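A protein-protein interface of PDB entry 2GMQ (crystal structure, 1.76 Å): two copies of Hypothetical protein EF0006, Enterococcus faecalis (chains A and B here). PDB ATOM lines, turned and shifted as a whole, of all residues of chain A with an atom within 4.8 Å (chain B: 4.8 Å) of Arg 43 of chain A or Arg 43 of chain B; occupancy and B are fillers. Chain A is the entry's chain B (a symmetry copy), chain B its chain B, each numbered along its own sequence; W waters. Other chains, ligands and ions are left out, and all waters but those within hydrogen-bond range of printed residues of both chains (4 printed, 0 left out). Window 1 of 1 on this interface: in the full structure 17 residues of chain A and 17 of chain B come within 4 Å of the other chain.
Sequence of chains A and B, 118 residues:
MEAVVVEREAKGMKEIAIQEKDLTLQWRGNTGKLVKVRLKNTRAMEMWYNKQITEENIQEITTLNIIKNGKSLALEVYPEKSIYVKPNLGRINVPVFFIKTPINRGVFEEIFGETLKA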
ATOM      1  N   ILE A  18     -14.684 -15.183  -0.920  1.00  0.00           N
ATOM      2  CA  ILE A  18     -13.717 -15.426   0.121  1.00  0.00           C
ATOM      3  C   ILE A  18     -13.271 -14.056   0.648  1.00  0.00           C
ATOM      4  O   ILE A  18     -12.913 -13.146  -0.165  1.00  0.00           O
ATOM      5  CB  ILE A  18     -12.466 -16.223  -0.442  1.00  0.00           C
ATOM      6  CG1 ILE A  18     -12.834 -17.590  -1.048  1.00  0.00           C
ATOM      7  CG2 ILE A  18     -11.466 -16.460   0.717  1.00  0.00           C
ATOM      8  CD1 ILE A  18     -11.669 -18.342  -1.721  1.00  0.00           C
ATOM      9  N   GLN A  19     -13.328 -13.837   1.957  1.00  0.00           N
ATOM     10  CA  GLN A  19     -12.857 -12.557   2.500  1.00  0.00           C
ATOM     11  C   GLN A  19     -11.369 -12.362   2.222  1.00  0.00           C
ATOM     12  O   GLN A  19     -10.569 -13.262   2.363  1.00  0.00           O
ATOM     13  CB  GLN A  19     -13.095 -12.414   4.021  1.00  0.00           C
ATOM     14  CG  GLN A  19     -12.782 -13.677   4.806  1.00  0.00           C
ATOM     15  CD  GLN A  19     -13.066 -13.556   6.348  1.00  0.00           C
ATOM     16  OE1 GLN A  19     -13.708 -12.594   6.849  1.00  0.00           O
ATOM     17  NE2 GLN A  19     -12.506 -14.510   7.103  1.00  0.00           N
ATOM     18  N   ASP A  22      -8.378 -13.619   4.309  1.00  0.00           N
ATOM     19  CA  ASP A  22      -7.959 -15.053   4.222  1.00  0.00           C
ATOM     20  C   ASP A  22      -7.080 -15.437   3.026  1.00  0.00           C
ATOM     21  O   ASP A  22      -6.796 -16.639   2.827  1.00  0.00           O
ATOM     22  CB  ASP A  22      -9.232 -15.986   4.249  1.00  0.00           C
ATOM     23  CG  ASP A  22      -9.798 -16.113   5.614  1.00  0.00           C
ATOM     24  OD1 ASP A  22      -9.113 -15.788   6.644  1.00  0.00           O
ATOM     25  OD2 ASP A  22     -10.986 -16.472   5.701  1.00  0.00           O
ATOM     26  N   LEU A  39      -4.926 -19.378  -0.359  1.00  0.00           N
ATOM     27  CA  LEU A  39      -5.594 -19.356   0.948  1.00  0.00           C
ATOM     28  C   LEU A  39      -4.587 -19.459   2.067  1.00  0.00           C
ATOM     29  O   LEU A  39      -3.593 -20.268   2.015  1.00  0.00           O
ATOM     30  CB  LEU A  39      -6.628 -20.476   1.103  1.00  0.00           C
ATOM     31  CG  LEU A  39      -8.032 -20.168   0.583  1.00  0.00           C
ATOM     32  CD1 LEU A  39      -8.708 -19.001   1.276  1.00  0.00           C
ATOM     33  CD2 LEU A  39      -7.995 -19.971  -0.888  1.00  0.00           C
ATOM     34  N   LYS A  40      -4.825 -18.642   3.079  1.00  0.00           N
ATOM     35  CA  LYS A  40      -4.099 -18.766   4.354  1.00  0.00           C
ATOM     36  C   LYS A  40      -4.273 -20.146   5.019  1.00  0.00           C
ATOM     37  O   LYS A  40      -5.294 -20.832   4.799  1.00  0.00           O
ATOM     38  CB  LYS A  40      -4.477 -17.635   5.307  1.00  0.00           C
ATOM     39  CG  LYS A  40      -4.174 -16.259   4.764  1.00  0.00           C
ATOM     40  CD  LYS A  40      -4.383 -15.179   5.842  1.00  0.00           C
ATOM     41  CE  LYS A  40      -3.429 -13.974   5.606  1.00  0.00           C
ATOM     42  NZ  LYS A  40      -4.118 -12.659   5.787  1.00  0.00           N
ATOM     43  N   ASN A  41      -3.270 -20.556   5.801  1.00  0.00           N
ATOM     44  CA  ASN A  41      -3.216 -21.884   6.398  1.00  0.00           C
ATOM     45  C   ASN A  41      -4.444 -22.159   7.284  1.00  0.00           C
ATOM     46  O   ASN A  41      -5.090 -23.197   7.127  1.00  0.00           O
ATOM     47  CB  ASN A  41      -1.940 -22.093   7.242  1.00  0.00           C
ATOM     48  CG  ASN A  41      -0.649 -22.084   6.421  1.00  0.00           C
ATOM     49  OD1 ASN A  41       0.419 -22.168   7.007  1.00  0.00           O
ATOM     50  ND2 ASN A  41      -0.732 -21.988   5.113  1.00  0.00           N
ATOM     51  N   THR A  42      -4.746 -21.249   8.203  1.00  0.00           N
ATOM     52  CA  THR A  42      -5.921 -21.452   9.118  1.00  0.00           C
ATOM     53  C   THR A  42      -7.267 -21.633   8.355  1.00  0.00           C
ATOM     54  O   THR A  42      -8.057 -22.565   8.646  1.00  0.00           O
ATOM     55  CB  THR A  42      -6.055 -20.266  10.127  1.00  0.00           C
ATOM     56  OG1 THR A  42      -4.826 -20.112  10.852  1.00  0.00           O
ATOM     57  CG2 THR A  42      -7.147 -20.572  11.212  1.00  0.00           C
ATOM     58  N   ARG A  43      -7.570 -20.707   7.457  1.00  0.00           N
ATOM     59  CA  ARG A  43      -8.791 -20.797   6.588  1.00  0.00           C
ATOM     60  C   ARG A  43      -8.725 -22.126   5.760  1.00  0.00           C
ATOM     61  O   ARG A  43      -9.713 -22.870   5.628  1.00  0.00           O
ATOM     62  CB  ARG A  43      -9.003 -19.538   5.731  1.00  0.00           C
ATOM     63  CG  ARG A  43     -10.395 -19.521   4.936  1.00  0.00           C
ATOM     64  CD  ARG A  43     -11.578 -19.849   5.900  1.00  0.00           C
ATOM     65  NE  ARG A  43     -12.857 -19.982   5.142  1.00  0.00           N
ATOM     66  CZ  ARG A  43     -13.563 -19.009   4.526  1.00  0.00           C
ATOM     67  NH1 ARG A  43     -13.136 -17.762   4.451  1.00  0.00           N
ATOM     68  NH2 ARG A  43     -14.699 -19.344   3.869  1.00  0.00           N
ATOM     69  N   ALA A  44      -7.574 -22.445   5.216  1.00  0.00           N
ATOM     70  CA  ALA A  44      -7.415 -23.740   4.479  1.00  0.00           C
ATOM     71  C   ALA A  44      -7.801 -24.948   5.366  1.00  0.00           C
ATOM     72  O   ALA A  44      -8.492 -25.889   4.913  1.00  0.00           O
ATOM     73  CB  ALA A  44      -6.026 -23.876   3.925  1.00  0.00           C
ATOM     74  N   MET A  45      -7.389 -24.909   6.645  1.00  0.00           N
ATOM     75  CA  MET A  45      -7.706 -25.984   7.599  1.00  0.00           C
ATOM     76  C   MET A  45      -9.205 -26.017   7.759  1.00  0.00           C
ATOM     77  O   MET A  45      -9.852 -27.037   7.694  1.00  0.00           O
ATOM     78  CB  MET A  45      -7.087 -25.681   8.964  1.00  0.00           C
ATOM     79  CG  MET A  45      -7.415 -26.720  10.077  1.00  0.00           C
ATOM     80  SD  MET A  45      -6.230 -26.628  11.689  1.00  0.00           S
ATOM     81  CE  MET A  45      -7.365 -27.246  13.091  1.00  0.00           C
ATOM     82  N   GLU A  46      -9.770 -24.850   8.025  1.00  0.00           N
ATOM     83  CA  GLU A  46     -11.232 -24.768   8.193  1.00  0.00           C
ATOM     84  C   GLU A  46     -11.966 -25.359   6.952  1.00  0.00           C
ATOM     85  O   GLU A  46     -12.893 -26.179   7.123  1.00  0.00           O
ATOM     86  CB  GLU A  46     -11.620 -23.299   8.374  1.00  0.00           C
ATOM     87  CG  GLU A  46     -13.070 -23.126   8.916  1.00  0.00           C
ATOM     88  CD  GLU A  46     -13.640 -21.869   8.376  1.00  0.00           C
ATOM     89  OE1 GLU A  46     -13.540 -20.867   9.111  1.00  0.00           O
ATOM     90  OE2 GLU A  46     -14.068 -21.832   7.193  1.00  0.00           O
ATOM     91  N   MET A  47     -11.617 -24.923   5.720  1.00  0.00           N
ATOM     92  CA  MET A  47     -12.183 -25.451   4.485  1.00  0.00           C
ATOM     93  C   MET A  47     -12.030 -26.970   4.334  1.00  0.00           C
ATOM     94  O   MET A  47     -12.959 -27.636   3.824  1.00  0.00           O
ATOM     95  CB  MET A  47     -11.546 -24.708   3.269  1.00  0.00           C
ATOM     96  CG  MET A  47     -11.958 -23.293   3.306  1.00  0.00           C
ATOM     97  SD  MET A  47     -11.172 -22.460   1.693  1.00  0.00           S
ATOM     98  CE  MET A  47     -12.379 -20.875   1.611  1.00  0.00           C
ATOM     99  N   GLN A  52     -15.368 -27.231   1.981  1.00  0.00           N
ATOM    100  CA  GLN A  52     -15.859 -26.056   1.278  1.00  0.00           C
ATOM    101  C   GLN A  52     -15.202 -25.958  -0.101  1.00  0.00           C
ATOM    102  O   GLN A  52     -15.875 -25.708  -1.122  1.00  0.00           O
ATOM    103  CB  GLN A  52     -15.632 -24.777   2.082  1.00  0.00           C
ATOM    104  CG  GLN A  52     -16.305 -23.620   1.320  1.00  0.00           C
ATOM    105  CD  GLN A  52     -16.309 -22.351   2.151  1.00  0.00           C
ATOM    106  OE1 GLN A  52     -15.539 -22.216   3.099  1.00  0.00           O
ATOM    107  NE2 GLN A  52     -17.240 -21.472   1.850  1.00  0.00           N
ATOM    108  N   ILE B  18     -15.244 -23.302  12.175  1.00  0.00           N
ATOM    109  CA  ILE B  18     -15.096 -21.894  11.904  1.00  0.00           C
ATOM    110  C   ILE B  18     -13.796 -21.442  12.581  1.00  0.00           C
ATOM    111  O   ILE B  18     -13.572 -21.744  13.796  1.00  0.00           O
ATOM    112  CB  ILE B  18     -16.323 -21.073  12.483  1.00  0.00           C
ATOM    113  CG1 ILE B  18     -17.681 -21.507  11.899  1.00  0.00           C
ATOM    114  CG2 ILE B  18     -16.114 -19.573  12.159  1.00  0.00           C
ATOM    115  CD1 ILE B  18     -18.911 -20.823  12.526  1.00  0.00           C
ATOM    116  N   GLN B  19     -12.901 -20.786  11.851  1.00  0.00           N
ATOM    117  CA  GLN B  19     -11.671 -20.291  12.481  1.00  0.00           C
ATOM    118  C   GLN B  19     -11.990 -19.266  13.566  1.00  0.00           C
ATOM    119  O   GLN B  19     -12.823 -18.400  13.402  1.00  0.00           O
ATOM    120  CB  GLN B  19     -10.684 -19.652  11.478  1.00  0.00           C
ATOM    121  CG  GLN B  19     -11.359 -18.767  10.443  1.00  0.00           C
ATOM    122  CD  GLN B  19     -10.368 -18.150   9.388  1.00  0.00           C
ATOM    123  OE1 GLN B  19      -9.174 -18.536   9.268  1.00  0.00           O
ATOM    124  NE2 GLN B  19     -10.862 -17.127   8.679  1.00  0.00           N
ATOM    125  N   ASP B  22     -12.550 -15.471  13.157  1.00  0.00           N
ATOM    126  CA  ASP B  22     -13.856 -14.962  12.631  1.00  0.00           C
ATOM    127  C   ASP B  22     -15.006 -14.862  13.641  1.00  0.00           C
ATOM    128  O   ASP B  22     -16.154 -14.561  13.243  1.00  0.00           O
ATOM    129  CB  ASP B  22     -14.320 -15.842  11.406  1.00  0.00           C
ATOM    130  CG  ASP B  22     -13.565 -15.518  10.172  1.00  0.00           C
ATOM    131  OD1 ASP B  22     -12.897 -14.431  10.075  1.00  0.00           O
ATOM    132  OD2 ASP B  22     -13.548 -16.382   9.276  1.00  0.00           O
ATOM    133  N   LEU B  39     -20.509 -14.416  14.715  1.00  0.00           N
ATOM    134  CA  LEU B  39     -19.640 -14.229  13.546  1.00  0.00           C
ATOM    135  C   LEU B  39     -19.344 -12.766  13.326  1.00  0.00           C
ATOM    136  O   LEU B  39     -20.250 -11.864  13.439  1.00  0.00           O
ATOM    137  CB  LEU B  39     -20.241 -14.814  12.264  1.00  0.00           C
ATOM    138  CG  LEU B  39     -19.960 -16.295  12.008  1.00  0.00           C
ATOM    139  CD1 LEU B  39     -18.488 -16.632  11.865  1.00  0.00           C
ATOM    140  CD2 LEU B  39     -20.599 -17.120  13.064  1.00  0.00           C
ATOM    141  N   LYS B  40     -18.083 -12.514  13.021  1.00  0.00           N
ATOM    142  CA  LYS B  40     -17.658 -11.189  12.540  1.00  0.00           C
ATOM    143  C   LYS B  40     -18.385 -10.749  11.253  1.00  0.00           C
ATOM    144  O   LYS B  40     -18.836 -11.600  10.457  1.00  0.00           O
ATOM    145  CB  LYS B  40     -16.142 -11.132  12.372  1.00  0.00           C
ATOM    146  CG  LYS B  40     -15.381 -11.397  13.649  1.00  0.00           C
ATOM    147  CD  LYS B  40     -13.876 -11.124  13.465  1.00  0.00           C
ATOM    148  CE  LYS B  40     -13.233 -10.662  14.803  1.00  0.00           C
ATOM    149  NZ  LYS B  40     -11.914 -11.319  15.058  1.00  0.00           N
ATOM    150  N   ASN B  41     -18.519  -9.432  11.071  1.00  0.00           N
ATOM    151  CA  ASN B  41     -19.291  -8.853   9.979  1.00  0.00           C
ATOM    152  C   ASN B  41     -18.767  -9.313   8.607  1.00  0.00           C
ATOM    153  O   ASN B  41     -19.553  -9.771   7.776  1.00  0.00           O
ATOM    154  CB  ASN B  41     -19.288  -7.309  10.017  1.00  0.00           C
ATOM    155  CG  ASN B  41     -20.007  -6.722  11.232  1.00  0.00           C
ATOM    156  OD1 ASN B  41     -19.995  -5.511  11.391  1.00  0.00           O
ATOM    157  ND2 ASN B  41     -20.614  -7.538  12.065  1.00  0.00           N
ATOM    158  N   THR B  42     -17.465  -9.180   8.377  1.00  0.00           N
ATOM    159  CA  THR B  42     -16.879  -9.592   7.056  1.00  0.00           C
ATOM    160  C   THR B  42     -17.140 -11.088   6.710  1.00  0.00           C
ATOM    161  O   THR B  42     -17.567 -11.427   5.579  1.00  0.00           O
ATOM    162  CB  THR B  42     -15.342  -9.313   7.016  1.00  0.00           C
ATOM    163  OG1 THR B  42     -15.097  -7.929   7.307  1.00  0.00           O
ATOM    164  CG2 THR B  42     -14.767  -9.546   5.574  1.00  0.00           C
ATOM    165  N   ARG B  43     -16.803 -11.978   7.632  1.00  0.00           N
ATOM    166  CA  ARG B  43     -17.074 -13.446   7.471  1.00  0.00           C
ATOM    167  C   ARG B  43     -18.615 -13.657   7.281  1.00  0.00           C
ATOM    168  O   ARG B  43     -19.074 -14.424   6.415  1.00  0.00           O
ATOM    169  CB  ARG B  43     -16.464 -14.290   8.603  1.00  0.00           C
ATOM    170  CG  ARG B  43     -16.571 -15.871   8.364  1.00  0.00           C
ATOM    171  CD  ARG B  43     -16.058 -16.243   6.937  1.00  0.00           C
ATOM    172  NE  ARG B  43     -16.292 -17.689   6.651  1.00  0.00           N
ATOM    173  CZ  ARG B  43     -15.676 -18.756   7.205  1.00  0.00           C
ATOM    174  NH1 ARG B  43     -14.795 -18.639   8.182  1.00  0.00           N
ATOM    175  NH2 ARG B  43     -16.051 -19.999   6.819  1.00  0.00           N
ATOM    176  N   ALA B  44     -19.421 -12.978   8.063  1.00  0.00           N
ATOM    177  CA  ALA B  44     -20.906 -13.067   7.885  1.00  0.00           C
ATOM    178  C   ALA B  44     -21.327 -12.701   6.441  1.00  0.00           C
ATOM    179  O   ALA B  44     -22.184 -13.376   5.826  1.00  0.00           O
ATOM    180  CB  ALA B  44     -21.621 -12.228   8.904  1.00  0.00           C
ATOM    181  N   MET B  45     -20.699 -11.655   5.880  1.00  0.00           N
ATOM    182  CA  MET B  45     -20.990 -11.214   4.506  1.00  0.00           C
ATOM    183  C   MET B  45     -20.600 -12.339   3.581  1.00  0.00           C
ATOM    184  O   MET B  45     -21.323 -12.748   2.702  1.00  0.00           O
ATOM    185  CB  MET B  45     -20.146  -9.990   4.152  1.00  0.00           C
ATOM    186  CG  MET B  45     -20.320  -9.476   2.691  1.00  0.00           C
ATOM    187  SD  MET B  45     -19.640  -7.620   2.367  1.00  0.00           S
ATOM    188  CE  MET B  45     -19.138  -7.663   0.528  1.00  0.00           C
ATOM    189  N   GLU B  46     -19.383 -12.826   3.765  1.00  0.00           N
ATOM    190  CA  GLU B  46     -18.903 -13.933   2.919  1.00  0.00           C
ATOM    191  C   GLU B  46     -19.890 -15.138   2.973  1.00  0.00           C
ATOM    192  O   GLU B  46     -20.260 -15.673   1.906  1.00  0.00           O
ATOM    193  CB  GLU B  46     -17.525 -14.368   3.421  1.00  0.00           C
ATOM    194  CG  GLU B  46     -16.773 -15.270   2.398  1.00  0.00           C
ATOM    195  CD  GLU B  46     -15.915 -16.226   3.137  1.00  0.00           C
ATOM    196  OE1 GLU B  46     -14.727 -15.883   3.291  1.00  0.00           O
ATOM    197  OE2 GLU B  46     -16.427 -17.244   3.671  1.00  0.00           O
ATOM    198  N   MET B  47     -20.275 -15.612   4.180  1.00  0.00           N
ATOM    199  CA  MET B  47     -21.244 -16.686   4.356  1.00  0.00           C
ATOM    200  C   MET B  47     -22.594 -16.417   3.680  1.00  0.00           C
ATOM    201  O   MET B  47     -23.206 -17.359   3.128  1.00  0.00           O
ATOM    202  CB  MET B  47     -21.434 -16.962   5.880  1.00  0.00           C
ATOM    203  CG  MET B  47     -20.172 -17.490   6.430  1.00  0.00           C
ATOM    204  SD  MET B  47     -20.535 -17.882   8.334  1.00  0.00           S
ATOM    205  CE  MET B  47     -19.023 -19.148   8.628  1.00  0.00           C
ATOM    206  N   GLN B  52     -23.337 -20.415   3.218  1.00  0.00           N
ATOM    207  CA  GLN B  52     -22.650 -21.387   4.055  1.00  0.00           C
ATOM    208  C   GLN B  52     -23.457 -21.641   5.330  1.00  0.00           C
ATOM    209  O   GLN B  52     -23.654 -22.800   5.752  1.00  0.00           O
ATOM    210  CB  GLN B  52     -21.227 -20.943   4.390  1.00  0.00           C
ATOM    211  CG  GLN B  52     -20.548 -22.093   5.157  1.00  0.00           C
ATOM    212  CD  GLN B  52     -19.067 -21.820   5.345  1.00  0.00           C
ATOM    213  OE1 GLN B  52     -18.617 -20.682   5.239  1.00  0.00           O
ATOM    214  NE2 GLN B  52     -18.308 -22.880   5.527  1.00  0.00           N
HETATM  215  O   HOH W   1     -15.117 -23.604   5.475  1.00  0.00           O
HETATM  216  O   HOH W   2     -14.187 -11.917   9.220  1.00  0.00           O
HETATM  217  O   HOH W   3      -7.242 -17.696   7.900  1.00  0.00           O
HETATM  218  O   HOH W   4     -18.562 -18.796   3.192  1.00  0.00           O
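Of chain B, only Gln 19 (3.3 Å), Arg 43 (3.3 Å) and Glu 46 (2.7 Å) come within 4 Å of Arg 43 of chain A.
Of the printed residues of chain A, Ile 18 of chain B touches Glu 46 (3.4 Å).
Printed residues of chain A within 4 Å of Thr 42 of chain B: Gln 19 (3.5 Å).
Of the printed residues of chain A, Asp 22 of chain B touches Gln 19 (3.0 Å).
Of the printed residues of chain A, Glu 46 of chain B touches Ile 18, Gln 19 and Arg 43.
Ala 44 of chain A touches none of the printed residues of chain B.
Lys 40 of chain A touches none of the printed residues of chain B.
The nearest residue of chain B that does not touch Arg 43 of chain A is Gln 52 of chain B (4.4 Å).
The nearest residue of chain A that does not touch Arg 43 of chain B is Gln 52 of chain A (4.4 Å).
Ile 18 of chain A touches Glu 46 of chain B, and with the chains exchanged Glu 46 of chain A touches Ile 18 of chain B.
Gln 19 of chain B touches its own counterpart, Gln 19 of chain A.
Gln 19 of chain A touches Glu 46 of chain B, and with the chains exchanged Glu 46 of chain A touches Gln 19 of chain B.
Gln 52 of chain A touches its own counterpart, Gln 52 of chain B.
Positions printed for both chains: 18, 19, 22, 39, 40, 41, 42, 43, 44, 45, 46, 47 and 52.
OD2 of Asp 22 of chain B lies within hydrogen-bond range of NE2 of Gln 19 of chain B, 2.9 Å away.
O of Asp 22 of chain B sits at hydrogen-bond distance from N of Lys 40 of chain B (2.8 Å).
The side-chain amide nitrogen (NE2) of Gln 19 of chain A lies within hydrogen-bond range of the side-chain carboxylate (OD2) of Asp 22 of chain A (2.9 Å).
The side-chain carboxylate of Asp 22 of chain B lies within salt-bridge range of the guanidinium group of Arg 43 of chain B (2.8 Å).
O of Met 47 of chain A is in hydrogen-bond range of N of Gln 52 of chain A (3.1 Å).
O of Asp 22 of chain A lies within hydrogen-bond range of N of Lys 40 of chain A (2.8 Å).
OE1 of Gln 19 of chain B sits at hydrogen-bond distance from N of Arg 43 of chain A, at 3.3 Å.
The guanidinium group of Arg 43 of chain B lies within salt-bridge range of the side-chain carboxylate of Glu 46 of chain A (2.7 Å).
The side-chain carboxylate (OE1) of Glu 46 of chain B is in salt-bridge range of the guanidinium group (NH1) of Arg 43 of chain A, 2.7 Å away.
NE2 of Gln 19 of chain A lies close to NE2 of Gln 19 of chain B.
OD1 of Asp 22 of chain B sits at hydrogen-bond distance from NE2 of Gln 19 of chain A (3.0 Å).
The backbone NH (N) of Gln 19 of chain B is in hydrogen-bond range of the side-chain carboxylate (OE1) of Glu 46 of chain A (2.8 Å).
OE1 of Glu 46 of chain B lies within hydrogen-bond range of N of Gln 19 of chain A (2.8 Å).
The guanidinium group of Arg 43 of chain A lies close to the guanidinium group of Arg 43 of chain B, at 3.3 Å.
The side-chain amide nitrogen (NE2) of Gln 19 of chain B sits at hydrogen-bond distance from the side-chain carboxylate (OD1) of Asp 22 of chain A (3.0 Å).
OE1 of Gln 19 of chain A lies within hydrogen-bond range of N of Arg 43 of chain B (3.3 Å).
Among the printed residues, pairs that only touch across the chains: Glu 46 of chain A with Ile 18 of chain B (3.4 Å), Ile 18 of chain A with Glu 46 of chain B (3.4 Å), Thr 42 of chain A with Gln 19 of chain B (3.5 Å), Gln 19 of chain A with Thr 42 of chain B (3.5 Å) and Gln 52 of chain A with Gln 52 of chain B (3.7 Å).
Of the 13 printed residues of chain A, 7 touch a printed residue of chain B.
Water W2 lies within hydrogen-bond range of the side-chain amide oxygen (OE1) of Gln 19 of chain A (2.5 Å), the side-chain carboxylate (OD1) of Asp 22 of chain B (3.0 Å) and the backbone NH (N) of Arg 43 of chain B (3.1 Å).
Water W3 lies within hydrogen-bond range of OE1 of Gln 19 of chain B, OD1 of Asp 22 of chain A and N of Arg 43 of chain A.
Water W4 lies within hydrogen-bond range of the side-chain carboxylate (OE2) of Glu 46 of chain B, the side-chain amide oxygen (OE1) of Gln 52 of chain B and the side-chain amide nitrogen (NE2) of Gln 52 of chain A.
Water W1 lies within hydrogen-bond range of OE2 of Glu 46 of chain A, OE1 of Gln 52 of chain A and NE2 of Gln 52 of chain B.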
